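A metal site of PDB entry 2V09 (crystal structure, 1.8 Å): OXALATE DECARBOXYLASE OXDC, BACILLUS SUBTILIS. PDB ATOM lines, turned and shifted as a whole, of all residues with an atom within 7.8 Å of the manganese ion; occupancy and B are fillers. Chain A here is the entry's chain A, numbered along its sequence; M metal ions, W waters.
The side-chain carboxylate (OE2) of Glu 280 is in hydrogen-bond range of the side-chain amide nitrogen (NE2) of Gln 282 (2.8 Å). The backbone carbonyl oxygen (O) of Glu 280 sits at hydrogen-bond distance from the backbone NH (N) of Val 313, at 2.8 Å. A ring nitrogen (ND1) of His 275 is in hydrogen-bond range of the backbone carbonyl oxygen (O) of Ala 341 (2.8 Å). The guanidinium group (NH2) of Arg 270 sits close to a ring nitrogen (NE2) of His 273 (3.4 Å). A ring nitrogen (ND1) of His 273 sits at hydrogen-bond distance from the backbone carbonyl oxygen (O) of Glu 271 (2.7 Å). ND1 of His 319 lies within hydrogen-bond range of O of Met 317, at 2.9 Å. OE2 of Glu 333 is in salt-bridge range of NE of Arg 270 (2.9 Å). OH of Tyr 340 is in hydrogen-bond range of OE1 of Glu 333 (2.8 Å).
Residues that only touch the manganese ion: Glu 333 (3.5 Å). Within 4 Å of the manganese ion: His 273, His 275, Glu 280, His 319 and Glu 333. Along chain A the residues within 4 Å of the manganese ion span positions 273 to 333.
The manganese ion is bound by OE1 of Glu 280 (2.1 Å), NE2 of His 275 (2.2 Å), water W1 (2.2 Å), NE2 of His 273 (2.2 Å) and NE2 of His 319 (2.3 Å). The manganese ion has five donor atoms within binding distance.
Water W1 lies within hydrogen-bond range of the side-chain carboxylate (OE2) of Glu 333 and the side-chain carboxylate (OE2) of Glu 280.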
ATOM      1  N   VAL A 262      31.912  14.257  18.871  1.00  0.00           N
ATOM      2  CA  VAL A 262      30.986  13.411  19.566  1.00  0.00           C
ATOM      3  C   VAL A 262      31.639  12.827  20.835  1.00  0.00           C
ATOM      4  O   VAL A 262      32.724  12.272  20.765  1.00  0.00           O
ATOM      5  CB  VAL A 262      30.522  12.257  18.626  1.00  0.00           C
ATOM      6  CG1 VAL A 262      29.483  11.328  19.333  1.00  0.00           C
ATOM      7  CG2 VAL A 262      30.029  12.797  17.211  1.00  0.00           C
ATOM      8  N   ARG A 270      26.558   6.108  19.665  1.00  0.00           N
ATOM      9  CA  ARG A 270      26.089   7.011  18.606  1.00  0.00           C
ATOM     10  C   ARG A 270      25.096   6.113  17.840  1.00  0.00           C
ATOM     11  O   ARG A 270      25.432   5.008  17.412  1.00  0.00           O
ATOM     12  CB  ARG A 270      27.248   7.464  17.701  1.00  0.00           C
ATOM     13  CG  ARG A 270      26.858   8.321  16.546  1.00  0.00           C
ATOM     14  CD  ARG A 270      26.648   9.783  16.888  1.00  0.00           C
ATOM     15  NE  ARG A 270      26.427  10.571  15.685  1.00  0.00           N
ATOM     16  CZ  ARG A 270      25.230  10.702  15.083  1.00  0.00           C
ATOM     17  NH1 ARG A 270      24.126  10.135  15.547  1.00  0.00           N
ATOM     18  NH2 ARG A 270      25.159  11.419  13.952  1.00  0.00           N
ATOM     19  N   GLU A 271      23.867   6.574  17.810  1.00  0.00           N
ATOM     20  CA  GLU A 271      22.729   5.791  17.314  1.00  0.00           C
ATOM     21  C   GLU A 271      22.868   5.375  15.829  1.00  0.00           C
ATOM     22  O   GLU A 271      23.666   5.932  15.091  1.00  0.00           O
ATOM     23  CB  GLU A 271      21.417   6.588  17.506  1.00  0.00           C
ATOM     24  CG  GLU A 271      21.194   7.755  16.552  1.00  0.00           C
ATOM     25  CD  GLU A 271      19.775   8.349  16.539  1.00  0.00           C
ATOM     26  OE1 GLU A 271      18.838   7.684  17.044  1.00  0.00           O
ATOM     27  OE2 GLU A 271      19.621   9.468  16.002  1.00  0.00           O
ATOM     28  N   HIS A 273      22.325   5.548  12.209  1.00  0.00           N
ATOM     29  CA  HIS A 273      22.081   6.713  11.343  1.00  0.00           C
ATOM     30  C   HIS A 273      22.823   6.559   9.997  1.00  0.00           C
ATOM     31  O   HIS A 273      23.655   5.627   9.802  1.00  0.00           O
ATOM     32  CB  HIS A 273      22.472   7.997  12.082  1.00  0.00           C
ATOM     33  CG  HIS A 273      23.956   8.188  12.263  1.00  0.00           C
ATOM     34  ND1 HIS A 273      24.690   7.514  13.221  1.00  0.00           N
ATOM     35  CD2 HIS A 273      24.845   8.931  11.568  1.00  0.00           C
ATOM     36  CE1 HIS A 273      25.960   7.859  13.133  1.00  0.00           C
ATOM     37  NE2 HIS A 273      26.080   8.709  12.114  1.00  0.00           N
ATOM     38  N   TRP A 274      22.539   7.466   9.067  1.00  0.00           N
ATOM     39  CA  TRP A 274      23.410   7.657   7.929  1.00  0.00           C
ATOM     40  C   TRP A 274      23.468   9.147   7.610  1.00  0.00           C
ATOM     41  O   TRP A 274      22.725   9.968   8.189  1.00  0.00           O
ATOM     42  CB  TRP A 274      22.993   6.826   6.687  1.00  0.00           C
ATOM     43  CG  TRP A 274      21.766   7.291   5.986  1.00  0.00           C
ATOM     44  CD1 TRP A 274      21.703   8.157   4.939  1.00  0.00           C
ATOM     45  CD2 TRP A 274      20.424   6.863   6.236  1.00  0.00           C
ATOM     46  NE1 TRP A 274      20.404   8.321   4.540  1.00  0.00           N
ATOM     47  CE2 TRP A 274      19.588   7.530   5.311  1.00  0.00           C
ATOM     48  CE3 TRP A 274      19.847   6.000   7.187  1.00  0.00           C
ATOM     49  CZ2 TRP A 274      18.201   7.381   5.301  1.00  0.00           C
ATOM     50  CZ3 TRP A 274      18.481   5.839   7.179  1.00  0.00           C
ATOM     51  CH2 TRP A 274      17.662   6.497   6.215  1.00  0.00           C
ATOM     52  N   HIS A 275      24.403   9.467   6.718  1.00  0.00           N
ATOM     53  CA  HIS A 275      24.567  10.831   6.178  1.00  0.00           C
ATOM     54  C   HIS A 275      24.122  10.865   4.724  1.00  0.00           C
ATOM     55  O   HIS A 275      24.660  10.135   3.887  1.00  0.00           O
ATOM     56  CB  HIS A 275      26.009  11.309   6.377  1.00  0.00           C
ATOM     57  CG  HIS A 275      26.444  11.218   7.797  1.00  0.00           C
ATOM     58  ND1 HIS A 275      26.014  12.112   8.751  1.00  0.00           N
ATOM     59  CD2 HIS A 275      27.136  10.259   8.458  1.00  0.00           C
ATOM     60  CE1 HIS A 275      26.438  11.714   9.945  1.00  0.00           C
ATOM     61  NE2 HIS A 275      27.138  10.607   9.795  1.00  0.00           N
ATOM     62  N   GLU A 280      31.755  10.120   5.473  1.00  0.00           N
ATOM     63  CA  GLU A 280      32.249  10.497   6.779  1.00  0.00           C
ATOM     64  C   GLU A 280      33.695   9.993   6.949  1.00  0.00           C
ATOM     65  O   GLU A 280      33.973   8.856   6.706  1.00  0.00           O
ATOM     66  CB  GLU A 280      31.409   9.841   7.903  1.00  0.00           C
ATOM     67  CG  GLU A 280      31.880  10.202   9.295  1.00  0.00           C
ATOM     68  CD  GLU A 280      30.941   9.634  10.361  1.00  0.00           C
ATOM     69  OE1 GLU A 280      29.751   9.648  10.118  1.00  0.00           O
ATOM     70  OE2 GLU A 280      31.388   9.180  11.428  1.00  0.00           O
ATOM     71  N   TRP A 281      34.553  10.897   7.406  1.00  0.00           N
ATOM     72  CA  TRP A 281      35.903  10.575   7.833  1.00  0.00           C
ATOM     73  C   TRP A 281      35.919  10.770   9.357  1.00  0.00           C
ATOM     74  O   TRP A 281      35.373  11.762   9.887  1.00  0.00           O
ATOM     75  CB  TRP A 281      36.888  11.509   7.118  1.00  0.00           C
ATOM     76  CG  TRP A 281      38.317  11.312   7.359  1.00  0.00           C
ATOM     77  CD1 TRP A 281      39.216  10.643   6.564  1.00  0.00           C
ATOM     78  CD2 TRP A 281      39.052  11.791   8.489  1.00  0.00           C
ATOM     79  NE1 TRP A 281      40.459  10.670   7.116  1.00  0.00           N
ATOM     80  CE2 TRP A 281      40.389  11.375   8.295  1.00  0.00           C
ATOM     81  CE3 TRP A 281      38.728  12.527   9.641  1.00  0.00           C
ATOM     82  CZ2 TRP A 281      41.400  11.629   9.254  1.00  0.00           C
ATOM     83  CZ3 TRP A 281      39.771  12.819  10.593  1.00  0.00           C
ATOM     84  CH2 TRP A 281      41.085  12.350  10.367  1.00  0.00           C
ATOM     85  N   GLN A 282      36.551   9.830  10.059  1.00  0.00           N
ATOM     86  CA  GLN A 282      36.548   9.806  11.524  1.00  0.00           C
ATOM     87  C   GLN A 282      37.945   9.859  12.080  1.00  0.00           C
ATOM     88  O   GLN A 282      38.844   9.251  11.526  1.00  0.00           O
ATOM     89  CB  GLN A 282      35.894   8.549  12.080  1.00  0.00           C
ATOM     90  CG  GLN A 282      34.530   8.207  11.497  1.00  0.00           C
ATOM     91  CD  GLN A 282      33.989   6.857  12.032  1.00  0.00           C
ATOM     92  OE1 GLN A 282      34.748   5.925  12.302  1.00  0.00           O
ATOM     93  NE2 GLN A 282      32.677   6.765  12.181  1.00  0.00           N
ATOM     94  N   MET A 291      32.115  -0.159  15.302  1.00  0.00           N
ATOM     95  CA  MET A 291      31.153   0.355  14.351  1.00  0.00           C
ATOM     96  C   MET A 291      30.929  -0.711  13.295  1.00  0.00           C
ATOM     97  O   MET A 291      31.903  -1.249  12.787  1.00  0.00           O
ATOM     98  CB  MET A 291      31.682   1.645  13.673  1.00  0.00           C
ATOM     99  CG  MET A 291      30.980   2.036  12.413  1.00  0.00           C
ATOM    100  SD  MET A 291      31.399   3.637  11.680  1.00  0.00           S
ATOM    101  CE  MET A 291      33.033   3.214  10.978  1.00  0.00           C
ATOM    102  N   VAL A 313      33.257   6.112   6.645  1.00  0.00           N
ATOM    103  CA  VAL A 313      31.962   5.593   6.304  1.00  0.00           C
ATOM    104  C   VAL A 313      31.598   6.178   4.958  1.00  0.00           C
ATOM    105  O   VAL A 313      31.291   7.345   4.886  1.00  0.00           O
ATOM    106  CB  VAL A 313      30.824   5.950   7.310  1.00  0.00           C
ATOM    107  CG1 VAL A 313      29.505   5.217   6.859  1.00  0.00           C
ATOM    108  CG2 VAL A 313      31.196   5.620   8.792  1.00  0.00           C
ATOM    109  N   MET A 317      26.085   5.051   3.732  1.00  0.00           N
ATOM    110  CA  MET A 317      26.134   3.738   4.397  1.00  0.00           C
ATOM    111  C   MET A 317      25.605   3.837   5.849  1.00  0.00           C
ATOM    112  O   MET A 317      25.855   4.799   6.570  1.00  0.00           O
ATOM    113  CB  MET A 317      27.550   3.129   4.353  1.00  0.00           C
ATOM    114  CG  MET A 317      27.957   2.716   2.924  1.00  0.00           C
ATOM    115  SD  MET A 317      29.370   1.660   2.889  1.00  0.00           S
ATOM    116  CE  MET A 317      29.477   1.365   1.084  1.00  0.00           C
ATOM    117  N   GLY A 318      24.862   2.824   6.272  1.00  0.00           N
ATOM    118  CA  GLY A 318      24.230   2.837   7.584  1.00  0.00           C
ATOM    119  C   GLY A 318      25.326   2.518   8.593  1.00  0.00           C
ATOM    120  O   GLY A 318      26.201   1.696   8.335  1.00  0.00           O
ATOM    121  N   HIS A 319      25.289   3.193   9.745  1.00  0.00           N
ATOM    122  CA  HIS A 319      26.227   2.893  10.817  1.00  0.00           C
ATOM    123  C   HIS A 319      25.776   3.384  12.236  1.00  0.00           C
ATOM    124  O   HIS A 319      24.753   4.082  12.397  1.00  0.00           O
ATOM    125  CB  HIS A 319      27.610   3.483  10.444  1.00  0.00           C
ATOM    126  CG  HIS A 319      27.598   4.955  10.232  1.00  0.00           C
ATOM    127  ND1 HIS A 319      26.976   5.553   9.152  1.00  0.00           N
ATOM    128  CD2 HIS A 319      28.148   5.958  10.948  1.00  0.00           C
ATOM    129  CE1 HIS A 319      27.119   6.867   9.242  1.00  0.00           C
ATOM    130  NE2 HIS A 319      27.849   7.141  10.303  1.00  0.00           N
ATOM    131  N   TYR A 320      26.531   2.905  13.224  1.00  0.00           N
ATOM    132  CA  TYR A 320      26.417   3.300  14.622  1.00  0.00           C
ATOM    133  C   TYR A 320      27.856   3.291  15.151  1.00  0.00           C
ATOM    134  O   TYR A 320      28.744   2.681  14.556  1.00  0.00           O
ATOM    135  CB  TYR A 320      25.553   2.298  15.386  1.00  0.00           C
ATOM    136  CG  TYR A 320      26.210   0.949  15.506  1.00  0.00           C
ATOM    137  CD1 TYR A 320      27.073   0.651  16.574  1.00  0.00           C
ATOM    138  CD2 TYR A 320      25.984  -0.038  14.559  1.00  0.00           C
ATOM    139  CE1 TYR A 320      27.704  -0.610  16.661  1.00  0.00           C
ATOM    140  CE2 TYR A 320      26.633  -1.274  14.617  1.00  0.00           C
ATOM    141  CZ  TYR A 320      27.472  -1.573  15.680  1.00  0.00           C
ATOM    142  OH  TYR A 320      28.074  -2.813  15.705  1.00  0.00           O
ATOM    143  N   VAL A 321      28.078   3.943  16.290  1.00  0.00           N
ATOM    144  CA  VAL A 321      29.406   3.871  16.932  1.00  0.00           C
ATOM    145  C   VAL A 321      29.174   3.601  18.422  1.00  0.00           C
ATOM    146  O   VAL A 321      28.678   4.458  19.125  1.00  0.00           O
ATOM    147  CB  VAL A 321      30.250   5.151  16.733  1.00  0.00           C
ATOM    148  CG1 VAL A 321      31.670   4.924  17.256  1.00  0.00           C
ATOM    149  CG2 VAL A 321      30.228   5.661  15.244  1.00  0.00           C
ATOM    150  N   PHE A 331      35.253  11.197  19.571  1.00  0.00           N
ATOM    151  CA  PHE A 331      35.664  11.129  18.188  1.00  0.00           C
ATOM    152  C   PHE A 331      35.050  12.284  17.384  1.00  0.00           C
ATOM    153  O   PHE A 331      34.117  12.951  17.781  1.00  0.00           O
ATOM    154  CB  PHE A 331      35.358   9.764  17.587  1.00  0.00           C
ATOM    155  CG  PHE A 331      33.893   9.459  17.401  1.00  0.00           C
ATOM    156  CD1 PHE A 331      33.180   8.809  18.391  1.00  0.00           C
ATOM    157  CD2 PHE A 331      33.251   9.748  16.172  1.00  0.00           C
ATOM    158  CE1 PHE A 331      31.821   8.492  18.220  1.00  0.00           C
ATOM    159  CE2 PHE A 331      31.916   9.449  16.000  1.00  0.00           C
ATOM    160  CZ  PHE A 331      31.193   8.798  17.035  1.00  0.00           C
ATOM    161  N   GLU A 333      33.587  13.428  13.532  1.00  0.00           N
ATOM    162  CA  GLU A 333      32.897  13.055  12.293  1.00  0.00           C
ATOM    163  C   GLU A 333      33.160  14.226  11.355  1.00  0.00           C
ATOM    164  O   GLU A 333      32.727  15.360  11.654  1.00  0.00           O
ATOM    165  CB  GLU A 333      31.368  12.907  12.466  1.00  0.00           C
ATOM    166  CG  GLU A 333      30.939  11.904  13.438  1.00  0.00           C
ATOM    167  CD  GLU A 333      29.429  11.943  13.745  1.00  0.00           C
ATOM    168  OE1 GLU A 333      28.753  13.040  13.610  1.00  0.00           O
ATOM    169  OE2 GLU A 333      28.948  10.889  14.202  1.00  0.00           O
ATOM    170  N   ILE A 334      33.847  13.950  10.253  1.00  0.00           N
ATOM    171  CA  ILE A 334      34.257  14.982   9.304  1.00  0.00           C
ATOM    172  C   ILE A 334      33.674  14.693   7.895  1.00  0.00           C
ATOM    173  O   ILE A 334      33.678  13.555   7.438  1.00  0.00           O
ATOM    174  CB  ILE A 334      35.818  15.052   9.209  1.00  0.00           C
ATOM    175  CG1 ILE A 334      36.453  15.249  10.611  1.00  0.00           C
ATOM    176  CG2 ILE A 334      36.226  16.137   8.223  1.00  0.00           C
ATOM    177  CD1 ILE A 334      36.063  16.564  11.295  1.00  0.00           C
ATOM    178  N   PHE A 335      33.267  15.749   7.196  1.00  0.00           N
ATOM    179  CA  PHE A 335      32.587  15.655   5.897  1.00  0.00           C
ATOM    180  C   PHE A 335      33.099  16.750   4.965  1.00  0.00           C
ATOM    181  O   PHE A 335      33.207  17.884   5.373  1.00  0.00           O
ATOM    182  CB  PHE A 335      31.066  15.845   6.080  1.00  0.00           C
ATOM    183  CG  PHE A 335      30.463  14.916   7.082  1.00  0.00           C
ATOM    184  CD1 PHE A 335      30.442  15.246   8.451  1.00  0.00           C
ATOM    185  CD2 PHE A 335      29.967  13.692   6.683  1.00  0.00           C
ATOM    186  CE1 PHE A 335      29.947  14.334   9.379  1.00  0.00           C
ATOM    187  CE2 PHE A 335      29.482  12.785   7.642  1.00  0.00           C
ATOM    188  CZ  PHE A 335      29.456  13.119   8.939  1.00  0.00           C
ATOM    189  N   TYR A 340      26.558  19.846   7.755  1.00  0.00           N
ATOM    190  CA  TYR A 340      26.384  18.607   8.461  1.00  0.00           C
ATOM    191  C   TYR A 340      24.917  18.149   8.295  1.00  0.00           C
ATOM    192  O   TYR A 340      24.007  18.949   8.491  1.00  0.00           O
ATOM    193  CB  TYR A 340      26.672  18.797   9.953  1.00  0.00           C
ATOM    194  CG  TYR A 340      26.546  17.512  10.720  1.00  0.00           C
ATOM    195  CD1 TYR A 340      25.334  17.081  11.206  1.00  0.00           C
ATOM    196  CD2 TYR A 340      27.644  16.703  10.893  1.00  0.00           C
ATOM    197  CE1 TYR A 340      25.215  15.869  11.908  1.00  0.00           C
ATOM    198  CE2 TYR A 340      27.538  15.473  11.597  1.00  0.00           C
ATOM    199  CZ  TYR A 340      26.316  15.075  12.106  1.00  0.00           C
ATOM    200  OH  TYR A 340      26.192  13.887  12.805  1.00  0.00           O
ATOM    201  N   ALA A 341      24.695  16.867   7.955  1.00  0.00           N
ATOM    202  CA  ALA A 341      23.328  16.342   7.949  1.00  0.00           C
ATOM    203  C   ALA A 341      23.362  14.864   8.325  1.00  0.00           C
ATOM    204  O   ALA A 341      24.275  14.139   7.937  1.00  0.00           O
ATOM    205  CB  ALA A 341      22.706  16.493   6.569  1.00  0.00           C
ATOM    206  N   ASP A 342      22.357  14.428   9.082  1.00  0.00           N
ATOM    207  CA  ASP A 342      22.181  13.000   9.339  1.00  0.00           C
ATOM    208  C   ASP A 342      20.688  12.636   9.271  1.00  0.00           C
ATOM    209  O   ASP A 342      19.797  13.493   9.426  1.00  0.00           O
ATOM    210  CB  ASP A 342      22.874  12.519  10.640  1.00  0.00           C
ATOM    211  CG  ASP A 342      22.267  13.124  11.968  1.00  0.00           C
ATOM    212  OD1 ASP A 342      21.457  14.087  11.953  1.00  0.00           O
ATOM    213  OD2 ASP A 342      22.651  12.640  13.061  1.00  0.00           O
HETATM  214 MN    MN M   1      28.027   9.224  11.215  1.00  0.00          MN
HETATM  215  O   HOH W   1      29.244   8.639  12.919  1.00  0.00           O
